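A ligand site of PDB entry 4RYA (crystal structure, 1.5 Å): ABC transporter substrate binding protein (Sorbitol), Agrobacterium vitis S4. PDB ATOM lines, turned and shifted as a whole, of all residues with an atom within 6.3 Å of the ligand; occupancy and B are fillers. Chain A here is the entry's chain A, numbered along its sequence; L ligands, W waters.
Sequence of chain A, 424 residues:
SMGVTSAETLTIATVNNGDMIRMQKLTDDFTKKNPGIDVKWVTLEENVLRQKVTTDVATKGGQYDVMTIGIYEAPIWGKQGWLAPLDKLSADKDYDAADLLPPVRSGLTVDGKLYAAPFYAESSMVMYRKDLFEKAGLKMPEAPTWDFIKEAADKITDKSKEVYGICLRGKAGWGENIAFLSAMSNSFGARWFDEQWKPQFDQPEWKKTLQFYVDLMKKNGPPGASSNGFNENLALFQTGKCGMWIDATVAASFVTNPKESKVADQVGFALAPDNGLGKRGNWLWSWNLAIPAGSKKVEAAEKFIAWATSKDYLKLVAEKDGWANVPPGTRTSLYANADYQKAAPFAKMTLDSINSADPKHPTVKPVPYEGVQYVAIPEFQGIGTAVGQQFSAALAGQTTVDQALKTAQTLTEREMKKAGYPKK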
ATOM      1  N   VAL A  15      23.171 -16.080   2.185  1.00  0.00           N
ATOM      2  CA  VAL A  15      22.755 -14.846   2.825  1.00  0.00           C
ATOM      3  C   VAL A  15      24.009 -13.932   3.021  1.00  0.00           C
ATOM      4  O   VAL A  15      25.136 -14.388   3.287  1.00  0.00           O
ATOM      5  CB  VAL A  15      22.036 -15.139   4.172  1.00  0.00           C
ATOM      6  CG1 VAL A  15      22.902 -15.969   5.102  1.00  0.00           C
ATOM      7  CG2 VAL A  15      21.605 -13.853   4.862  1.00  0.00           C
ATOM      8  N   ASN A  17      25.269 -12.421   5.412  1.00  0.00           N
ATOM      9  CA  ASN A  17      25.719 -12.282   6.790  1.00  0.00           C
ATOM     10  C   ASN A  17      27.225 -12.421   6.914  1.00  0.00           C
ATOM     11  O   ASN A  17      27.882 -13.031   6.088  1.00  0.00           O
ATOM     12  CB  ASN A  17      25.056 -13.235   7.744  1.00  0.00           C
ATOM     13  CG  ASN A  17      23.596 -12.933   7.996  1.00  0.00           C
ATOM     14  OD1 ASN A  17      23.048 -11.899   7.603  1.00  0.00           O
ATOM     15  ND2 ASN A  17      22.927 -13.911   8.621  1.00  0.00           N
ATOM     16  N   GLU A  46      18.375 -11.874   3.549  1.00  0.00           N
ATOM     17  CA  GLU A  46      17.695 -13.124   3.913  1.00  0.00           C
ATOM     18  C   GLU A  46      16.245 -13.213   3.425  1.00  0.00           C
ATOM     19  O   GLU A  46      15.808 -14.284   3.007  1.00  0.00           O
ATOM     20  CB  GLU A  46      17.794 -13.415   5.420  1.00  0.00           C
ATOM     21  CG  GLU A  46      17.134 -12.445   6.393  1.00  0.00           C
ATOM     22  CD  GLU A  46      17.424 -12.884   7.806  1.00  0.00           C
ATOM     23  OE1 GLU A  46      18.620 -13.066   8.134  1.00  0.00           O
ATOM     24  OE2 GLU A  46      16.450 -13.138   8.547  1.00  0.00           O
ATOM     25  N   ARG A  50      15.288 -16.358   0.823  1.00  0.00           N
ATOM     26  CA  ARG A  50      14.235 -17.320   1.125  1.00  0.00           C
ATOM     27  C   ARG A  50      13.250 -17.496  -0.025  1.00  0.00           C
ATOM     28  O   ARG A  50      12.861 -18.620  -0.375  1.00  0.00           O
ATOM     29  CB  ARG A  50      13.534 -16.935   2.430  1.00  0.00           C
ATOM     30  CG  ARG A  50      14.427 -17.192   3.633  1.00  0.00           C
ATOM     31  CD  ARG A  50      14.028 -16.349   4.855  1.00  0.00           C
ATOM     32  NE  ARG A  50      14.829 -16.788   5.984  1.00  0.00           N
ATOM     33  CZ  ARG A  50      15.123 -16.029   7.037  1.00  0.00           C
ATOM     34  NH1 ARG A  50      14.575 -14.823   7.165  1.00  0.00           N
ATOM     35  NH2 ARG A  50      15.948 -16.497   7.968  1.00  0.00           N
ATOM     36  N   TYR A 120      26.367 -22.293  10.755  1.00  0.00           N
ATOM     37  CA  TYR A 120      26.403 -21.779  12.120  1.00  0.00           C
ATOM     38  C   TYR A 120      25.031 -21.882  12.733  1.00  0.00           C
ATOM     39  O   TYR A 120      24.041 -21.966  12.009  1.00  0.00           O
ATOM     40  CB  TYR A 120      26.973 -20.372  12.250  1.00  0.00           C
ATOM     41  CG  TYR A 120      26.139 -19.183  11.806  1.00  0.00           C
ATOM     42  CD1 TYR A 120      25.039 -18.739  12.543  1.00  0.00           C
ATOM     43  CD2 TYR A 120      26.513 -18.424  10.697  1.00  0.00           C
ATOM     44  CE1 TYR A 120      24.335 -17.628  12.151  1.00  0.00           C
ATOM     45  CE2 TYR A 120      25.830 -17.274  10.331  1.00  0.00           C
ATOM     46  CZ  TYR A 120      24.755 -16.873  11.044  1.00  0.00           C
ATOM     47  OH  TYR A 120      24.092 -15.713  10.670  1.00  0.00           O
ATOM     48  N   GLU A 122      22.596 -20.578  16.412  1.00  0.00           N
ATOM     49  CA  GLU A 122      22.423 -19.473  17.332  1.00  0.00           C
ATOM     50  C   GLU A 122      21.200 -19.639  18.217  1.00  0.00           C
ATOM     51  O   GLU A 122      20.274 -20.351  17.878  1.00  0.00           O
ATOM     52  CB  GLU A 122      22.234 -18.180  16.528  1.00  0.00           C
ATOM     53  CG  GLU A 122      20.880 -18.111  15.831  1.00  0.00           C
ATOM     54  CD  GLU A 122      20.719 -16.980  14.857  1.00  0.00           C
ATOM     55  OE1 GLU A 122      21.690 -16.646  14.166  1.00  0.00           O
ATOM     56  OE2 GLU A 122      19.602 -16.447  14.791  1.00  0.00           O
ATOM     57  N   ARG A 169      14.677  -5.650  15.905  1.00  0.00           N
ATOM     58  CA  ARG A 169      14.237  -5.839  14.528  1.00  0.00           C
ATOM     59  C   ARG A 169      12.921  -5.160  14.318  1.00  0.00           C
ATOM     60  O   ARG A 169      11.997  -5.361  15.078  1.00  0.00           O
ATOM     61  CB  ARG A 169      14.019  -7.282  14.169  1.00  0.00           C
ATOM     62  CG  ARG A 169      15.261  -8.082  14.423  1.00  0.00           C
ATOM     63  CD  ARG A 169      15.180  -9.387  13.743  1.00  0.00           C
ATOM     64  NE  ARG A 169      16.432 -10.088  13.972  1.00  0.00           N
ATOM     65  CZ  ARG A 169      16.643 -11.268  13.458  1.00  0.00           C
ATOM     66  NH1 ARG A 169      15.676 -11.854  12.728  1.00  0.00           N
ATOM     67  NH2 ARG A 169      17.755 -11.879  13.731  1.00  0.00           N
ATOM     68  N   TRP A 174       9.103 -12.858   7.390  1.00  0.00           N
ATOM     69  CA  TRP A 174       8.751 -13.962   8.270  1.00  0.00           C
ATOM     70  C   TRP A 174       9.874 -14.309   9.236  1.00  0.00           C
ATOM     71  O   TRP A 174       9.631 -14.692  10.357  1.00  0.00           O
ATOM     72  CB  TRP A 174       8.245 -15.202   7.522  1.00  0.00           C
ATOM     73  CG  TRP A 174       9.254 -16.039   6.743  1.00  0.00           C
ATOM     74  CD1 TRP A 174       9.451 -16.025   5.394  1.00  0.00           C
ATOM     75  CD2 TRP A 174      10.135 -17.042   7.257  1.00  0.00           C
ATOM     76  NE1 TRP A 174      10.412 -16.937   5.039  1.00  0.00           N
ATOM     77  CE2 TRP A 174      10.837 -17.583   6.175  1.00  0.00           C
ATOM     78  CE3 TRP A 174      10.388 -17.543   8.542  1.00  0.00           C
ATOM     79  CZ2 TRP A 174      11.800 -18.577   6.320  1.00  0.00           C
ATOM     80  CZ3 TRP A 174      11.336 -18.528   8.685  1.00  0.00           C
ATOM     81  CH2 TRP A 174      12.028 -19.032   7.584  1.00  0.00           C
ATOM     82  N   GLY A 175      11.111 -14.213   8.753  1.00  0.00           N
ATOM     83  CA  GLY A 175      12.268 -14.488   9.578  1.00  0.00           C
ATOM     84  C   GLY A 175      13.016 -13.285  10.086  1.00  0.00           C
ATOM     85  O   GLY A 175      14.083 -13.420  10.672  1.00  0.00           O
ATOM     86  N   GLU A 176      12.463 -12.088   9.860  1.00  0.00           N
ATOM     87  CA  GLU A 176      13.081 -10.857  10.352  1.00  0.00           C
ATOM     88  C   GLU A 176      12.308 -10.342  11.562  1.00  0.00           C
ATOM     89  O   GLU A 176      12.506 -10.844  12.650  1.00  0.00           O
ATOM     90  CB  GLU A 176      13.217  -9.801   9.241  1.00  0.00           C
ATOM     91  CG  GLU A 176      14.390 -10.024   8.279  1.00  0.00           C
ATOM     92  CD  GLU A 176      15.700  -9.407   8.753  1.00  0.00           C
ATOM     93  OE1 GLU A 176      15.797  -9.110   9.955  1.00  0.00           O
ATOM     94  OE2 GLU A 176      16.612  -9.237   7.925  1.00  0.00           O
ATOM     95  N   ALA A 179      10.457 -13.164  13.478  1.00  0.00           N
ATOM     96  CA  ALA A 179      11.301 -14.007  14.350  1.00  0.00           C
ATOM     97  C   ALA A 179      11.422 -13.379  15.723  1.00  0.00           C
ATOM     98  O   ALA A 179      11.134 -13.992  16.752  1.00  0.00           O
ATOM     99  CB  ALA A 179      12.662 -14.228  13.745  1.00  0.00           C
ATOM    100  N   PHE A 230      18.229  -7.644  10.938  1.00  0.00           N
ATOM    101  CA  PHE A 230      19.392  -8.074  11.700  1.00  0.00           C
ATOM    102  C   PHE A 230      20.626  -7.245  11.356  1.00  0.00           C
ATOM    103  O   PHE A 230      21.315  -6.756  12.252  1.00  0.00           O
ATOM    104  CB  PHE A 230      19.636  -9.568  11.448  1.00  0.00           C
ATOM    105  CG  PHE A 230      20.932 -10.073  12.014  1.00  0.00           C
ATOM    106  CD1 PHE A 230      21.109 -10.233  13.376  1.00  0.00           C
ATOM    107  CD2 PHE A 230      21.996 -10.339  11.182  1.00  0.00           C
ATOM    108  CE1 PHE A 230      22.322 -10.670  13.898  1.00  0.00           C
ATOM    109  CE2 PHE A 230      23.207 -10.783  11.681  1.00  0.00           C
ATOM    110  CZ  PHE A 230      23.375 -10.947  13.041  1.00  0.00           C
ATOM    111  N   ASP A 247      19.050  -9.950  20.289  1.00  0.00           N
ATOM    112  CA  ASP A 247      19.087 -10.599  18.983  1.00  0.00           C
ATOM    113  C   ASP A 247      20.024 -11.798  19.014  1.00  0.00           C
ATOM    114  O   ASP A 247      20.373 -12.308  20.061  1.00  0.00           O
ATOM    115  CB  ASP A 247      19.526  -9.543  17.916  1.00  0.00           C
ATOM    116  CG  ASP A 247      18.885  -9.745  16.552  1.00  0.00           C
ATOM    117  OD1 ASP A 247      18.966 -10.854  15.992  1.00  0.00           O
ATOM    118  OD2 ASP A 247      18.255  -8.777  16.035  1.00  0.00           O
ATOM    119  N   ALA A 248      20.291 -12.313  17.804  1.00  0.00           N
ATOM    120  CA  ALA A 248      21.027 -13.537  17.596  1.00  0.00           C
ATOM    121  C   ALA A 248      22.373 -13.610  18.290  1.00  0.00           C
ATOM    122  O   ALA A 248      23.166 -12.654  18.194  1.00  0.00           O
ATOM    123  CB  ALA A 248      21.212 -13.719  16.108  1.00  0.00           C
ATOM    124  N   VAL A 250      24.901 -15.178  17.331  1.00  0.00           N
ATOM    125  CA  VAL A 250      26.002 -15.106  16.345  1.00  0.00           C
ATOM    126  C   VAL A 250      26.653 -13.721  16.306  1.00  0.00           C
ATOM    127  O   VAL A 250      27.843 -13.606  16.029  1.00  0.00           O
ATOM    128  CB  VAL A 250      25.562 -15.581  14.957  1.00  0.00           C
ATOM    129  CG1 VAL A 250      24.546 -14.623  14.353  1.00  0.00           C
ATOM    130  CG2 VAL A 250      26.766 -15.747  14.041  1.00  0.00           C
ATOM    131  N   TRP A 283      15.607 -18.131  21.134  1.00  0.00           N
ATOM    132  CA  TRP A 283      15.207 -18.947  19.990  1.00  0.00           C
ATOM    133  C   TRP A 283      16.284 -19.953  19.607  1.00  0.00           C
ATOM    134  O   TRP A 283      17.342 -20.081  20.251  1.00  0.00           O
ATOM    135  CB  TRP A 283      14.781 -18.058  18.814  1.00  0.00           C
ATOM    136  CG  TRP A 283      15.806 -17.231  18.072  1.00  0.00           C
ATOM    137  CD1 TRP A 283      16.849 -17.682  17.307  1.00  0.00           C
ATOM    138  CD2 TRP A 283      15.784 -15.804  17.928  1.00  0.00           C
ATOM    139  NE1 TRP A 283      17.467 -16.627  16.705  1.00  0.00           N
ATOM    140  CE2 TRP A 283      16.847 -15.464  17.068  1.00  0.00           C
ATOM    141  CE3 TRP A 283      14.959 -14.794  18.403  1.00  0.00           C
ATOM    142  CZ2 TRP A 283      17.146 -14.150  16.719  1.00  0.00           C
ATOM    143  CZ3 TRP A 283      15.264 -13.496  18.097  1.00  0.00           C
ATOM    144  CH2 TRP A 283      16.328 -13.177  17.225  1.00  0.00           C
ATOM    145  N   LEU A 284      15.975 -20.770  18.615  1.00  0.00           N
ATOM    146  CA  LEU A 284      16.960 -21.686  18.030  1.00  0.00           C
ATOM    147  C   LEU A 284      16.896 -21.527  16.516  1.00  0.00           C
ATOM    148  O   LEU A 284      15.845 -21.752  15.858  1.00  0.00           O
ATOM    149  CB  LEU A 284      16.660 -23.149  18.405  1.00  0.00           C
ATOM    150  CG  LEU A 284      17.691 -24.157  17.873  1.00  0.00           C
ATOM    151  CD1 LEU A 284      19.094 -23.949  18.466  1.00  0.00           C
ATOM    152  CD2 LEU A 284      17.173 -25.581  18.089  1.00  0.00           C
ATOM    153  N   TRP A 285      18.022 -21.101  15.934  1.00  0.00           N
ATOM    154  CA  TRP A 285      18.125 -20.981  14.480  1.00  0.00           C
ATOM    155  C   TRP A 285      19.449 -21.579  14.045  1.00  0.00           C
ATOM    156  O   TRP A 285      20.423 -21.509  14.770  1.00  0.00           O
ATOM    157  CB  TRP A 285      18.010 -19.524  13.998  1.00  0.00           C
ATOM    158  CG  TRP A 285      18.154 -19.316  12.546  1.00  0.00           C
ATOM    159  CD1 TRP A 285      19.263 -18.927  11.843  1.00  0.00           C
ATOM    160  CD2 TRP A 285      17.140 -19.618  11.567  1.00  0.00           C
ATOM    161  NE1 TRP A 285      18.983 -18.963  10.505  1.00  0.00           N
ATOM    162  CE2 TRP A 285      17.679 -19.334  10.310  1.00  0.00           C
ATOM    163  CE3 TRP A 285      15.819 -20.041  11.659  1.00  0.00           C
ATOM    164  CZ2 TRP A 285      16.948 -19.489   9.146  1.00  0.00           C
ATOM    165  CZ3 TRP A 285      15.080 -20.167  10.484  1.00  0.00           C
ATOM    166  CH2 TRP A 285      15.648 -19.905   9.274  1.00  0.00           C
ATOM    167  N   TRP A 287      21.730 -21.637  10.207  1.00  0.00           N
ATOM    168  CA  TRP A 287      21.951 -21.511   8.765  1.00  0.00           C
ATOM    169  C   TRP A 287      22.753 -22.702   8.283  1.00  0.00           C
ATOM    170  O   TRP A 287      23.804 -22.989   8.833  1.00  0.00           O
ATOM    171  CB  TRP A 287      22.671 -20.222   8.438  1.00  0.00           C
ATOM    172  CG  TRP A 287      21.797 -18.968   8.459  1.00  0.00           C
ATOM    173  CD1 TRP A 287      21.892 -17.934   9.331  1.00  0.00           C
ATOM    174  CD2 TRP A 287      20.790 -18.595   7.516  1.00  0.00           C
ATOM    175  NE1 TRP A 287      21.015 -16.949   8.983  1.00  0.00           N
ATOM    176  CE2 TRP A 287      20.309 -17.338   7.881  1.00  0.00           C
ATOM    177  CE3 TRP A 287      20.206 -19.247   6.418  1.00  0.00           C
ATOM    178  CZ2 TRP A 287      19.326 -16.690   7.151  1.00  0.00           C
ATOM    179  CZ3 TRP A 287      19.236 -18.587   5.700  1.00  0.00           C
ATOM    180  CH2 TRP A 287      18.800 -17.326   6.061  1.00  0.00           C
ATOM    181  N   GLN A 373      10.585 -19.155  17.330  1.00  0.00           N
ATOM    182  CA  GLN A 373      10.421 -17.882  16.623  1.00  0.00           C
ATOM    183  C   GLN A 373       9.701 -17.974  15.297  1.00  0.00           C
ATOM    184  O   GLN A 373       9.504 -16.965  14.625  1.00  0.00           O
ATOM    185  CB  GLN A 373      11.792 -17.189  16.433  1.00  0.00           C
ATOM    186  CG  GLN A 373      12.713 -17.732  15.333  1.00  0.00           C
ATOM    187  CD  GLN A 373      13.455 -19.029  15.634  1.00  0.00           C
ATOM    188  OE1 GLN A 373      13.004 -19.860  16.421  1.00  0.00           O
ATOM    189  NE2 GLN A 373      14.580 -19.239  14.936  1.00  0.00           N
ATOM    190  N   TYR A 374       9.424 -19.206  14.872  1.00  0.00           N
ATOM    191  CA  TYR A 374       8.642 -19.516  13.723  1.00  0.00           C
ATOM    192  C   TYR A 374       7.626 -20.591  14.102  1.00  0.00           C
ATOM    193  O   TYR A 374       7.719 -21.193  15.157  1.00  0.00           O
ATOM    194  CB  TYR A 374       9.538 -19.917  12.545  1.00  0.00           C
ATOM    195  CG  TYR A 374      10.403 -21.116  12.781  1.00  0.00           C
ATOM    196  CD1 TYR A 374       9.893 -22.424  12.725  1.00  0.00           C
ATOM    197  CD2 TYR A 374      11.729 -20.952  13.085  1.00  0.00           C
ATOM    198  CE1 TYR A 374      10.713 -23.502  12.942  1.00  0.00           C
ATOM    199  CE2 TYR A 374      12.551 -22.024  13.326  1.00  0.00           C
ATOM    200  CZ  TYR A 374      12.038 -23.302  13.275  1.00  0.00           C
ATOM    201  OH  TYR A 374      12.871 -24.382  13.487  1.00  0.00           O
HETATM  202  O1  LIG L   1      21.862 -15.341  11.879  1.00  0.00           O
HETATM  203  C1  LIG L   1      21.286 -14.040  12.004  1.00  0.00           C
HETATM  204  C2  LIG L   1      19.974 -13.969  11.236  1.00  0.00           C
HETATM  205  O2  LIG L   1      20.195 -14.275   9.845  1.00  0.00           O
HETATM  206  C3  LIG L   1      18.969 -14.919  11.858  1.00  0.00           C
HETATM  207  O3  LIG L   1      18.751 -14.525  13.228  1.00  0.00           O
HETATM  208  C4  LIG L   1      17.650 -14.914  11.092  1.00  0.00           C
HETATM  209  O4  LIG L   1      17.036 -13.623  11.133  1.00  0.00           O
HETATM  210  C5  LIG L   1      16.624 -15.975  11.523  1.00  0.00           C
HETATM  211  O5  LIG L   1      15.424 -15.851  10.715  1.00  0.00           O
HETATM  212  C6  LIG L   1      16.215 -15.936  12.981  1.00  0.00           C
HETATM  213  O6  LIG L   1      15.255 -16.955  13.242  1.00  0.00           O
HETATM  214  O   HOH W   1      12.982 -17.661  11.844  1.00  0.00           O
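The backbone carbonyl oxygen (O) of Tyr 120 lies within hydrogen-bond range of the backbone NH (N) of Trp 287, 2.9 Å away. The side-chain amide nitrogen of Asn 17 is in hydrogen-bond range of the side-chain hydroxyl of Tyr 120, 3.0 Å away. N of Glu 122 lies within hydrogen-bond range of O of Trp 285 (2.9 Å). OE2 of Glu 46 is in salt-bridge range of NH1 of Arg 50 (2.9 Å). NH1 of Arg 169 is in hydrogen-bond range of O of Gly 175 (3.0 Å). The guanidinium group of Arg 169 is in salt-bridge range of the side-chain carboxylate of Asp 247, 2.8 Å away. The side-chain carboxylate of Glu 176 is in salt-bridge range of the guanidinium group of Arg 169 (3.9 Å). The backbone NH (N) of Phe 230 sits at hydrogen-bond distance from the side-chain carboxylate (OE1) of Glu 176 (3.0 Å).
O1 of the ligand is in hydrogen-bond range of OH of Tyr 120. OE2 of Glu 122 sits at hydrogen-bond distance from O3 of the ligand (2.6 Å). OE1 of Glu 46 sits at hydrogen-bond distance from O2 of the ligand (2.6 Å). An oxygen (O4) of the ligand is in hydrogen-bond range of the guanidinium group (NH1) of Arg 169, 2.7 Å away. The backbone carbonyl oxygen (O) of Gly 175 lies within hydrogen-bond range of an oxygen (O5) of the ligand (2.8 Å). The guanidinium group of Arg 50 is in hydrogen-bond range of an oxygen (O5) of the ligand (2.9 Å). The side-chain amide nitrogen (NE2) of Gln 373 lies within hydrogen-bond range of an oxygen (O6) of the ligand (2.9 Å). O2 of the ligand sits at hydrogen-bond distance from NE1 of Trp 287, 2.9 Å away. The side-chain amide nitrogen of Asn 17 sits at hydrogen-bond distance from an oxygen (O2) of the ligand.
Ala 179 touches the ligand (CB to O6, 3.8 Å). CE2 of Phe 230 touches C1 of the ligand (3.8 Å). Ala 248 touches the ligand (CB to O3, 3.9 Å). Val 250 touches the ligand (CG1 to O1, 3.7 Å). Trp 283 touches the ligand. Trp 285 touches the ligand. Hydrophobic or aromatic side chains within 4 Å of the ligand: Tyr 120, Ala 179, Phe 230, Ala 248, Val 250, Trp 283, Trp 285 and Trp 287. 15 residues have an atom within 4 Å of the ligand: Asn 17, Glu 46, Arg 50, Tyr 120, Glu 122, Arg 169, Gly 175, Ala 179, Phe 230, Ala 248, Val 250, Trp 283, Trp 285, Trp 287 and Gln 373. Along chain A the residues within 4 Å of the ligand span positions 17 to 373. The nearest printed residue that does not touch the ligand is Asp 247 (4.6 Å).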
